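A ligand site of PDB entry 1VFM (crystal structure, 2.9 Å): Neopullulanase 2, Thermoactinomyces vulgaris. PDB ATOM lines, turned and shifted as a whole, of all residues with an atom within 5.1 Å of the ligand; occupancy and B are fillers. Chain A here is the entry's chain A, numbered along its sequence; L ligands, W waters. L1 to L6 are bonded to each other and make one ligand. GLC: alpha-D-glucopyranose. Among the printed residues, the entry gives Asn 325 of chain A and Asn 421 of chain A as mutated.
An oxygen (O2) of GLC L1 is in hydrogen-bond range of the side-chain amide oxygen (OD1) of Asn 421 (2.5 Å).
An oxygen (O3) of GLC L1 sits at hydrogen-bond distance from a ring nitrogen (NE2) of His 420, 3.0 Å away.
O3 of GLC L2 lies within hydrogen-bond range of OD2 of Asp 465 (2.7 Å).
O5 of GLC L1 sits close to OD1 of Asn 325 (3.0 Å).
The guanidinium group (NH2) of Arg 469 sits at hydrogen-bond distance from an oxygen (O2) of GLC L2 (2.6 Å).
A ring nitrogen (NE2) of His 244 sits at hydrogen-bond distance from an oxygen (O6) of GLC L1, at 3.1 Å.
O2 of GLC L1 sits at hydrogen-bond distance from OE1 of Glu 354 (2.7 Å).
NH2 of Arg 469 is in salt-bridge range of OD2 of Asp 465.
N of Tyr 204 lies within hydrogen-bond range of ND1 of His 202 (2.9 Å).
The side-chain carboxylate (OE2) of Glu 354 is in salt-bridge range of the guanidinium group (NH1) of Arg 323 (3.5 Å).
The backbone NH (N) of Phe 286 sits at hydrogen-bond distance from the backbone carbonyl oxygen (O) of Met 293 (3.2 Å).
The backbone carbonyl oxygen (O) of His 420 lies within hydrogen-bond range of the guanidinium group (NE) of Arg 469 (3.1 Å).
NE2 of His 420 is in hydrogen-bond range of OH of Tyr 204.
The side-chain carboxylate of Glu 354 lies within hydrogen-bond range of the backbone NH of Val 326, at 2.8 Å.
CG of His 202 touches C2 of GLC L2, at 3.9 Å.
CE2 of Tyr 204 touches O3 of GLC L1, 3.2 Å away.
Phe 286 touches the ligand.
CG2 of Val 290 touches O6 of GLC L4, at 3.7 Å.
CE of Met 293 touches O5 of GLC L2, at 3.6 Å.
CG2 of Val 326 touches O3 of GLC L3 (3.3 Å).
Trp 356 touches the ligand.
Hydrophobic or aromatic side chains that line the ligand: His 202, Tyr 204, His 244, Phe 286, Val 290, Met 293, Val 326, Trp 356 and His 420.
Of the 19 residues printed, 14 come within 4 Å of the ligand.
Along chain A the residues within 4 Å of the ligand span positions 202 to 469.
The nearest printed residue that does not touch the ligand is Ala 287 (4.1 Å).
Water W1 lies within hydrogen-bond range of the guanidinium group of Arg 323 (2.5 Å), an oxygen (O2) of GLC L1 (2.8 Å), the side-chain carboxylate of Glu 354 (3.0 Å) and the side-chain hydroxyl of Tyr 204 (3.1 Å).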
ATOM      1  N   HIS A 202       3.386  21.159   5.343  1.00  0.00           N
ATOM      2  CA  HIS A 202       3.068  20.906   3.926  1.00  0.00           C
ATOM      3  C   HIS A 202       4.380  20.818   3.147  1.00  0.00           C
ATOM      4  O   HIS A 202       4.424  20.213   2.083  1.00  0.00           O
ATOM      5  CB  HIS A 202       2.181  22.013   3.365  1.00  0.00           C
ATOM      6  CG  HIS A 202       2.735  23.381   3.588  1.00  0.00           C
ATOM      7  ND1 HIS A 202       3.825  23.871   2.896  1.00  0.00           N
ATOM      8  CD2 HIS A 202       2.372  24.357   4.451  1.00  0.00           C
ATOM      9  CE1 HIS A 202       4.104  25.083   3.321  1.00  0.00           C
ATOM     10  NE2 HIS A 202       3.238  25.412   4.267  1.00  0.00           N
ATOM     11  N   TYR A 204       6.303  23.187   1.457  1.00  0.00           N
ATOM     12  CA  TYR A 204       6.535  23.900   0.194  1.00  0.00           C
ATOM     13  C   TYR A 204       7.629  24.975   0.356  1.00  0.00           C
ATOM     14  O   TYR A 204       8.115  25.542  -0.616  1.00  0.00           O
ATOM     15  CB  TYR A 204       5.231  24.512  -0.363  1.00  0.00           C
ATOM     16  CG  TYR A 204       4.393  23.521  -1.168  1.00  0.00           C
ATOM     17  CD1 TYR A 204       4.837  23.054  -2.406  1.00  0.00           C
ATOM     18  CD2 TYR A 204       3.194  23.009  -0.681  1.00  0.00           C
ATOM     19  CE1 TYR A 204       4.110  22.104  -3.129  1.00  0.00           C
ATOM     20  CE2 TYR A 204       2.462  22.057  -1.396  1.00  0.00           C
ATOM     21  CZ  TYR A 204       2.932  21.600  -2.611  1.00  0.00           C
ATOM     22  OH  TYR A 204       2.241  20.629  -3.286  1.00  0.00           O
ATOM     23  N   VAL A 241       9.657  21.663  -6.356  1.00  0.00           N
ATOM     24  CA  VAL A 241       9.348  23.037  -6.002  1.00  0.00           C
ATOM     25  C   VAL A 241      10.511  23.937  -6.390  1.00  0.00           C
ATOM     26  O   VAL A 241      11.228  24.414  -5.525  1.00  0.00           O
ATOM     27  CB  VAL A 241       9.122  23.193  -4.474  1.00  0.00           C
ATOM     28  CG1 VAL A 241       8.359  24.468  -4.196  1.00  0.00           C
ATOM     29  CG2 VAL A 241       8.392  21.970  -3.914  1.00  0.00           C
ATOM     30  N   HIS A 244      10.237  28.761  -5.948  1.00  0.00           N
ATOM     31  CA  HIS A 244      10.671  29.464  -4.749  1.00  0.00           C
ATOM     32  C   HIS A 244      11.345  28.496  -3.782  1.00  0.00           C
ATOM     33  O   HIS A 244      11.341  27.276  -3.984  1.00  0.00           O
ATOM     34  CB  HIS A 244       9.468  30.131  -4.089  1.00  0.00           C
ATOM     35  CG  HIS A 244       8.258  29.238  -4.017  1.00  0.00           C
ATOM     36  ND1 HIS A 244       8.088  28.299  -3.026  1.00  0.00           N
ATOM     37  CD2 HIS A 244       7.190  29.118  -4.841  1.00  0.00           C
ATOM     38  CE1 HIS A 244       6.957  27.640  -3.238  1.00  0.00           C
ATOM     39  NE2 HIS A 244       6.392  28.125  -4.333  1.00  0.00           N
ATOM     40  N   PHE A 286       6.733  34.003  -3.525  1.00  0.00           N
ATOM     41  CA  PHE A 286       5.666  33.321  -4.231  1.00  0.00           C
ATOM     42  C   PHE A 286       4.431  34.091  -3.803  1.00  0.00           C
ATOM     43  O   PHE A 286       4.373  34.571  -2.675  1.00  0.00           O
ATOM     44  CB  PHE A 286       5.601  31.868  -3.750  1.00  0.00           C
ATOM     45  CG  PHE A 286       4.215  31.273  -3.759  1.00  0.00           C
ATOM     46  CD1 PHE A 286       3.336  31.493  -2.706  1.00  0.00           C
ATOM     47  CD2 PHE A 286       3.808  30.469  -4.831  1.00  0.00           C
ATOM     48  CE1 PHE A 286       2.069  30.936  -2.719  1.00  0.00           C
ATOM     49  CE2 PHE A 286       2.539  29.903  -4.846  1.00  0.00           C
ATOM     50  CZ  PHE A 286       1.663  30.141  -3.787  1.00  0.00           C
ATOM     51  N   ALA A 287       3.459  34.227  -4.700  1.00  0.00           N
ATOM     52  CA  ALA A 287       2.238  34.944  -4.375  1.00  0.00           C
ATOM     53  C   ALA A 287       2.543  36.332  -3.852  1.00  0.00           C
ATOM     54  O   ALA A 287       3.364  37.044  -4.419  1.00  0.00           O
ATOM     55  CB  ALA A 287       1.430  34.179  -3.337  1.00  0.00           C
ATOM     56  N   VAL A 288       1.894  36.720  -2.765  1.00  0.00           N
ATOM     57  CA  VAL A 288       2.115  38.040  -2.194  1.00  0.00           C
ATOM     58  C   VAL A 288       2.403  38.034  -0.691  1.00  0.00           C
ATOM     59  O   VAL A 288       1.643  37.469   0.109  1.00  0.00           O
ATOM     60  CB  VAL A 288       0.909  38.981  -2.473  1.00  0.00           C
ATOM     61  CG1 VAL A 288       1.157  40.356  -1.856  1.00  0.00           C
ATOM     62  CG2 VAL A 288       0.697  39.102  -3.969  1.00  0.00           C
ATOM     63  N   VAL A 290       4.611  36.417   1.220  1.00  0.00           N
ATOM     64  CA  VAL A 290       4.803  35.141   1.887  1.00  0.00           C
ATOM     65  C   VAL A 290       6.315  35.044   2.183  1.00  0.00           C
ATOM     66  O   VAL A 290       7.103  34.582   1.352  1.00  0.00           O
ATOM     67  CB  VAL A 290       4.344  33.977   0.989  1.00  0.00           C
ATOM     68  CG1 VAL A 290       4.364  32.669   1.760  1.00  0.00           C
ATOM     69  CG2 VAL A 290       2.939  34.260   0.472  1.00  0.00           C
ATOM     70  N   MET A 293       8.746  31.917   1.656  1.00  0.00           N
ATOM     71  CA  MET A 293       9.018  31.400   0.325  1.00  0.00           C
ATOM     72  C   MET A 293       9.628  32.375  -0.677  1.00  0.00           C
ATOM     73  O   MET A 293       8.986  32.758  -1.661  1.00  0.00           O
ATOM     74  CB  MET A 293       7.731  30.821  -0.245  1.00  0.00           C
ATOM     75  CG  MET A 293       6.998  29.920   0.719  1.00  0.00           C
ATOM     76  SD  MET A 293       5.536  29.243  -0.021  1.00  0.00           S
ATOM     77  CE  MET A 293       5.365  27.683   0.853  1.00  0.00           C
ATOM     78  N   ARG A 323       6.465  16.434 -10.635  1.00  0.00           N
ATOM     79  CA  ARG A 323       5.238  17.214 -10.711  1.00  0.00           C
ATOM     80  C   ARG A 323       5.762  18.632 -10.436  1.00  0.00           C
ATOM     81  O   ARG A 323       6.149  18.956  -9.322  1.00  0.00           O
ATOM     82  CB  ARG A 323       4.258  16.787  -9.626  1.00  0.00           C
ATOM     83  CG  ARG A 323       2.800  17.113  -9.931  1.00  0.00           C
ATOM     84  CD  ARG A 323       2.622  18.561 -10.356  1.00  0.00           C
ATOM     85  NE  ARG A 323       2.967  19.531  -9.307  1.00  0.00           N
ATOM     86  CZ  ARG A 323       2.186  19.839  -8.275  1.00  0.00           C
ATOM     87  NH1 ARG A 323       2.599  20.736  -7.383  1.00  0.00           N
ATOM     88  NH2 ARG A 323       1.000  19.263  -8.139  1.00  0.00           N
ATOM     89  N   ASN A 325       5.650  22.056  -9.390  1.00  0.00           N
ATOM     90  CA  ASN A 325       4.884  22.994  -8.588  1.00  0.00           C
ATOM     91  C   ASN A 325       5.054  24.414  -9.111  1.00  0.00           C
ATOM     92  O   ASN A 325       6.169  24.863  -9.344  1.00  0.00           O
ATOM     93  CB  ASN A 325       5.360  22.924  -7.135  1.00  0.00           C
ATOM     94  CG  ASN A 325       4.749  24.006  -6.259  1.00  0.00           C
ATOM     95  OD1 ASN A 325       3.605  23.886  -5.821  1.00  0.00           O
ATOM     96  ND2 ASN A 325       5.502  25.076  -6.027  1.00  0.00           N
ATOM     97  N   VAL A 326       3.939  25.129  -9.295  1.00  0.00           N
ATOM     98  CA  VAL A 326       3.974  26.502  -9.778  1.00  0.00           C
ATOM     99  C   VAL A 326       4.815  26.632 -11.063  1.00  0.00           C
ATOM    100  O   VAL A 326       5.369  27.684 -11.387  1.00  0.00           O
ATOM    101  CB  VAL A 326       4.498  27.450  -8.649  1.00  0.00           C
ATOM    102  CG1 VAL A 326       5.250  28.619  -9.216  1.00  0.00           C
ATOM    103  CG2 VAL A 326       3.318  28.010  -7.841  1.00  0.00           C
ATOM    104  N   ASN A 328       4.479  27.356 -14.197  1.00  0.00           N
ATOM    105  CA  ASN A 328       4.410  28.554 -15.031  1.00  0.00           C
ATOM    106  C   ASN A 328       5.126  29.802 -14.556  1.00  0.00           C
ATOM    107  O   ASN A 328       5.121  30.807 -15.256  1.00  0.00           O
ATOM    108  CB  ASN A 328       2.945  28.885 -15.379  1.00  0.00           C
ATOM    109  CG  ASN A 328       2.085  29.124 -14.140  1.00  0.00           C
ATOM    110  OD1 ASN A 328       2.265  28.473 -13.111  1.00  0.00           O
ATOM    111  ND2 ASN A 328       1.129  30.039 -14.260  1.00  0.00           N
ATOM    112  N   GLU A 354       2.003  21.931 -13.251  1.00  0.00           N
ATOM    113  CA  GLU A 354       0.867  22.387 -12.472  1.00  0.00           C
ATOM    114  C   GLU A 354       0.541  23.813 -12.862  1.00  0.00           C
ATOM    115  O   GLU A 354       1.001  24.768 -12.228  1.00  0.00           O
ATOM    116  CB  GLU A 354       1.222  22.356 -10.987  1.00  0.00           C
ATOM    117  CG  GLU A 354       0.048  22.576 -10.059  1.00  0.00           C
ATOM    118  CD  GLU A 354       0.472  23.166  -8.741  1.00  0.00           C
ATOM    119  OE1 GLU A 354      -0.260  22.982  -7.756  1.00  0.00           O
ATOM    120  OE2 GLU A 354       1.532  23.838  -8.696  1.00  0.00           O
ATOM    121  N   TRP A 356      -2.689  26.451 -13.791  1.00  0.00           N
ATOM    122  CA  TRP A 356      -4.135  26.636 -13.747  1.00  0.00           C
ATOM    123  C   TRP A 356      -4.664  27.609 -14.793  1.00  0.00           C
ATOM    124  O   TRP A 356      -5.346  28.584 -14.482  1.00  0.00           O
ATOM    125  CB  TRP A 356      -4.588  27.093 -12.351  1.00  0.00           C
ATOM    126  CG  TRP A 356      -4.180  26.188 -11.203  1.00  0.00           C
ATOM    127  CD1 TRP A 356      -3.663  26.579  -9.999  1.00  0.00           C
ATOM    128  CD2 TRP A 356      -4.213  24.743 -11.170  1.00  0.00           C
ATOM    129  NE1 TRP A 356      -3.378  25.486  -9.219  1.00  0.00           N
ATOM    130  CE2 TRP A 356      -3.706  24.339  -9.909  1.00  0.00           C
ATOM    131  CE3 TRP A 356      -4.627  23.764 -12.069  1.00  0.00           C
ATOM    132  CZ2 TRP A 356      -3.592  22.993  -9.537  1.00  0.00           C
ATOM    133  CZ3 TRP A 356      -4.520  22.416 -11.688  1.00  0.00           C
ATOM    134  CH2 TRP A 356      -4.003  22.056 -10.436  1.00  0.00           C
ATOM    135  N   HIS A 420      -5.036  18.453  -2.289  1.00  0.00           N
ATOM    136  CA  HIS A 420      -4.824  18.931  -0.928  1.00  0.00           C
ATOM    137  C   HIS A 420      -5.057  20.437  -0.870  1.00  0.00           C
ATOM    138  O   HIS A 420      -4.789  21.078   0.148  1.00  0.00           O
ATOM    139  CB  HIS A 420      -3.397  18.615  -0.478  1.00  0.00           C
ATOM    140  CG  HIS A 420      -2.344  19.215  -1.353  1.00  0.00           C
ATOM    141  ND1 HIS A 420      -2.065  18.738  -2.617  1.00  0.00           N
ATOM    142  CD2 HIS A 420      -1.533  20.277  -1.155  1.00  0.00           C
ATOM    143  CE1 HIS A 420      -1.113  19.484  -3.152  1.00  0.00           C
ATOM    144  NE2 HIS A 420      -0.775  20.423  -2.294  1.00  0.00           N
ATOM    145  N   ASN A 421      -5.558  20.997  -1.962  1.00  0.00           N
ATOM    146  CA  ASN A 421      -5.837  22.429  -2.046  1.00  0.00           C
ATOM    147  C   ASN A 421      -7.327  22.705  -2.220  1.00  0.00           C
ATOM    148  O   ASN A 421      -7.724  23.830  -2.541  1.00  0.00           O
ATOM    149  CB  ASN A 421      -5.098  23.069  -3.217  1.00  0.00           C
ATOM    150  CG  ASN A 421      -3.599  23.036  -3.071  1.00  0.00           C
ATOM    151  OD1 ASN A 421      -2.877  22.682  -4.005  1.00  0.00           O
ATOM    152  ND2 ASN A 421      -3.115  23.416  -1.882  1.00  0.00           N
ATOM    153  N   ASP A 465      -8.293  23.466   2.503  1.00  0.00           N
ATOM    154  CA  ASP A 465      -7.128  23.659   3.353  1.00  0.00           C
ATOM    155  C   ASP A 465      -7.533  24.278   4.694  1.00  0.00           C
ATOM    156  O   ASP A 465      -8.084  25.387   4.738  1.00  0.00           O
ATOM    157  CB  ASP A 465      -6.147  24.599   2.641  1.00  0.00           C
ATOM    158  CG  ASP A 465      -4.712  24.311   3.001  1.00  0.00           C
ATOM    159  OD1 ASP A 465      -4.471  23.876   4.153  1.00  0.00           O
ATOM    160  OD2 ASP A 465      -3.827  24.540   2.132  1.00  0.00           O
ATOM    161  N   ARG A 469      -6.925  17.881   4.474  1.00  0.00           N
ATOM    162  CA  ARG A 469      -5.688  17.229   4.830  1.00  0.00           C
ATOM    163  C   ARG A 469      -5.789  16.440   6.138  1.00  0.00           C
ATOM    164  O   ARG A 469      -4.839  16.392   6.910  1.00  0.00           O
ATOM    165  CB  ARG A 469      -4.557  18.265   4.934  1.00  0.00           C
ATOM    166  CG  ARG A 469      -4.239  18.982   3.623  1.00  0.00           C
ATOM    167  CD  ARG A 469      -3.232  20.103   3.844  1.00  0.00           C
ATOM    168  NE  ARG A 469      -2.957  20.843   2.607  1.00  0.00           N
ATOM    169  CZ  ARG A 469      -2.138  21.891   2.526  1.00  0.00           C
ATOM    170  NH1 ARG A 469      -1.515  22.341   3.607  1.00  0.00           N
ATOM    171  NH2 ARG A 469      -1.970  22.507   1.358  1.00  0.00           N
HETATM  172  C1  GLC L   1       0.700  25.145  -5.426  1.00  0.00           C
HETATM  173  C2  GLC L   1       0.410  23.960  -4.506  1.00  0.00           C
HETATM  174  C3  GLC L   1      -0.033  24.500  -3.136  1.00  0.00           C
HETATM  175  C4  GLC L   1       1.080  25.354  -2.548  1.00  0.00           C
HETATM  176  C5  GLC L   1       1.470  26.478  -3.520  1.00  0.00           C
HETATM  177  C6  GLC L   1       2.732  27.175  -3.070  1.00  0.00           C
HETATM  178  O2  GLC L   1      -0.606  23.155  -5.060  1.00  0.00           O
HETATM  179  O3  GLC L   1      -0.335  23.429  -2.264  1.00  0.00           O
HETATM  180  O4  GLC L   1       0.624  25.942  -1.318  1.00  0.00           O
HETATM  181  O5  GLC L   1       1.734  25.964  -4.855  1.00  0.00           O
HETATM  182  O6  GLC L   1       3.893  26.457  -3.492  1.00  0.00           O
HETATM  183  C1  GLC L   2       1.400  25.781  -0.167  1.00  0.00           C
HETATM  184  C2  GLC L   2       0.565  25.087   0.893  1.00  0.00           C
HETATM  185  C3  GLC L   2      -0.605  25.983   1.297  1.00  0.00           C
HETATM  186  C4  GLC L   2      -0.187  27.433   1.651  1.00  0.00           C
HETATM  187  C5  GLC L   2       0.801  27.975   0.599  1.00  0.00           C
HETATM  188  C6  GLC L   2       1.469  29.306   0.913  1.00  0.00           C
HETATM  189  O2  GLC L   2       0.050  23.884   0.353  1.00  0.00           O
HETATM  190  O3  GLC L   2      -1.286  25.402   2.398  1.00  0.00           O
HETATM  191  O4  GLC L   2      -1.393  28.230   1.608  1.00  0.00           O
HETATM  192  O5  GLC L   2       1.856  27.022   0.349  1.00  0.00           O
HETATM  193  O6  GLC L   2       1.889  29.374   2.264  1.00  0.00           O
HETATM  194  C1  GLC L   3      -1.528  29.493  -7.621  1.00  0.00           C
HETATM  195  C2  GLC L   3      -0.417  28.629  -8.255  1.00  0.00           C
HETATM  196  C3  GLC L   3      -0.514  27.186  -7.758  1.00  0.00           C
HETATM  197  C4  GLC L   3      -0.387  27.187  -6.238  1.00  0.00           C
HETATM  198  C5  GLC L   3      -1.512  28.068  -5.648  1.00  0.00           C
HETATM  199  C6  GLC L   3      -1.410  28.200  -4.130  1.00  0.00           C
HETATM  200  O2  GLC L   3      -0.501  28.676  -9.681  1.00  0.00           O
HETATM  201  O3  GLC L   3       0.530  26.405  -8.323  1.00  0.00           O
HETATM  202  O4  GLC L   3      -0.492  25.842  -5.712  1.00  0.00           O
HETATM  203  O5  GLC L   3      -1.447  29.404  -6.194  1.00  0.00           O
HETATM  204  O6  GLC L   3      -2.320  29.178  -3.635  1.00  0.00           O
HETATM  205  C1  GLC L   4      -1.659  29.106   2.665  1.00  0.00           C
HETATM  206  C2  GLC L   4      -3.151  29.033   2.987  1.00  0.00           C
HETATM  207  C3  GLC L   4      -3.952  29.467   1.763  1.00  0.00           C
HETATM  208  C4  GLC L   4      -3.491  30.824   1.207  1.00  0.00           C
HETATM  209  C5  GLC L   4      -1.967  30.935   1.136  1.00  0.00           C
HETATM  210  C6  GLC L   4      -1.494  32.357   0.950  1.00  0.00           C
HETATM  211  O2  GLC L   4      -3.503  27.709   3.366  1.00  0.00           O
HETATM  212  O3  GLC L   4      -5.320  29.528   2.109  1.00  0.00           O
HETATM  213  O4  GLC L   4      -4.019  30.978  -0.126  1.00  0.00           O
HETATM  214  O5  GLC L   4      -1.339  30.447   2.342  1.00  0.00           O
HETATM  215  O6  GLC L   4      -0.276  32.391   0.228  1.00  0.00           O
HETATM  216  C1  GLC L   5      -5.325  31.446  -5.615  1.00  0.00           C
HETATM  217  C2  GLC L   5      -5.869  30.081  -6.073  1.00  0.00           C
HETATM  218  C3  GLC L   5      -4.717  29.203  -6.589  1.00  0.00           C
HETATM  219  C4  GLC L   5      -3.963  29.933  -7.716  1.00  0.00           C
HETATM  220  C5  GLC L   5      -3.546  31.364  -7.277  1.00  0.00           C
HETATM  221  C6  GLC L   5      -3.053  32.181  -8.456  1.00  0.00           C
HETATM  222  O2  GLC L   5      -6.538  29.444  -5.001  1.00  0.00           O
HETATM  223  O3  GLC L   5      -5.234  27.976  -7.085  1.00  0.00           O
HETATM  224  O4  GLC L   5      -2.798  29.145  -8.126  1.00  0.00           O
HETATM  225  O5  GLC L   5      -4.674  32.094  -6.711  1.00  0.00           O
HETATM  226  O6  GLC L   5      -3.657  33.470  -8.477  1.00  0.00           O
HETATM  227  C1  GLC L   6      -4.576  32.230  -0.439  1.00  0.00           C
HETATM  228  C2  GLC L   6      -5.934  32.025  -1.107  1.00  0.00           C
HETATM  229  C3  GLC L   6      -5.739  31.283  -2.432  1.00  0.00           C
HETATM  230  C4  GLC L   6      -4.777  32.070  -3.347  1.00  0.00           C
HETATM  231  C5  GLC L   6      -3.466  32.403  -2.596  1.00  0.00           C
HETATM  232  C6  GLC L   6      -2.590  33.384  -3.354  1.00  0.00           C
HETATM  233  O2  GLC L   6      -6.788  31.275  -0.255  1.00  0.00           O
HETATM  234  O3  GLC L   6      -6.992  31.102  -3.092  1.00  0.00           O
HETATM  235  O4  GLC L   6      -4.479  31.281  -4.514  1.00  0.00           O
HETATM  236  O5  GLC L   6      -3.737  32.995  -1.299  1.00  0.00           O
HETATM  237  O6  GLC L   6      -2.750  34.714  -2.869  1.00  0.00           O
HETATM  238  O   HOH W   1       0.614  20.791  -5.937  1.00  0.00           O
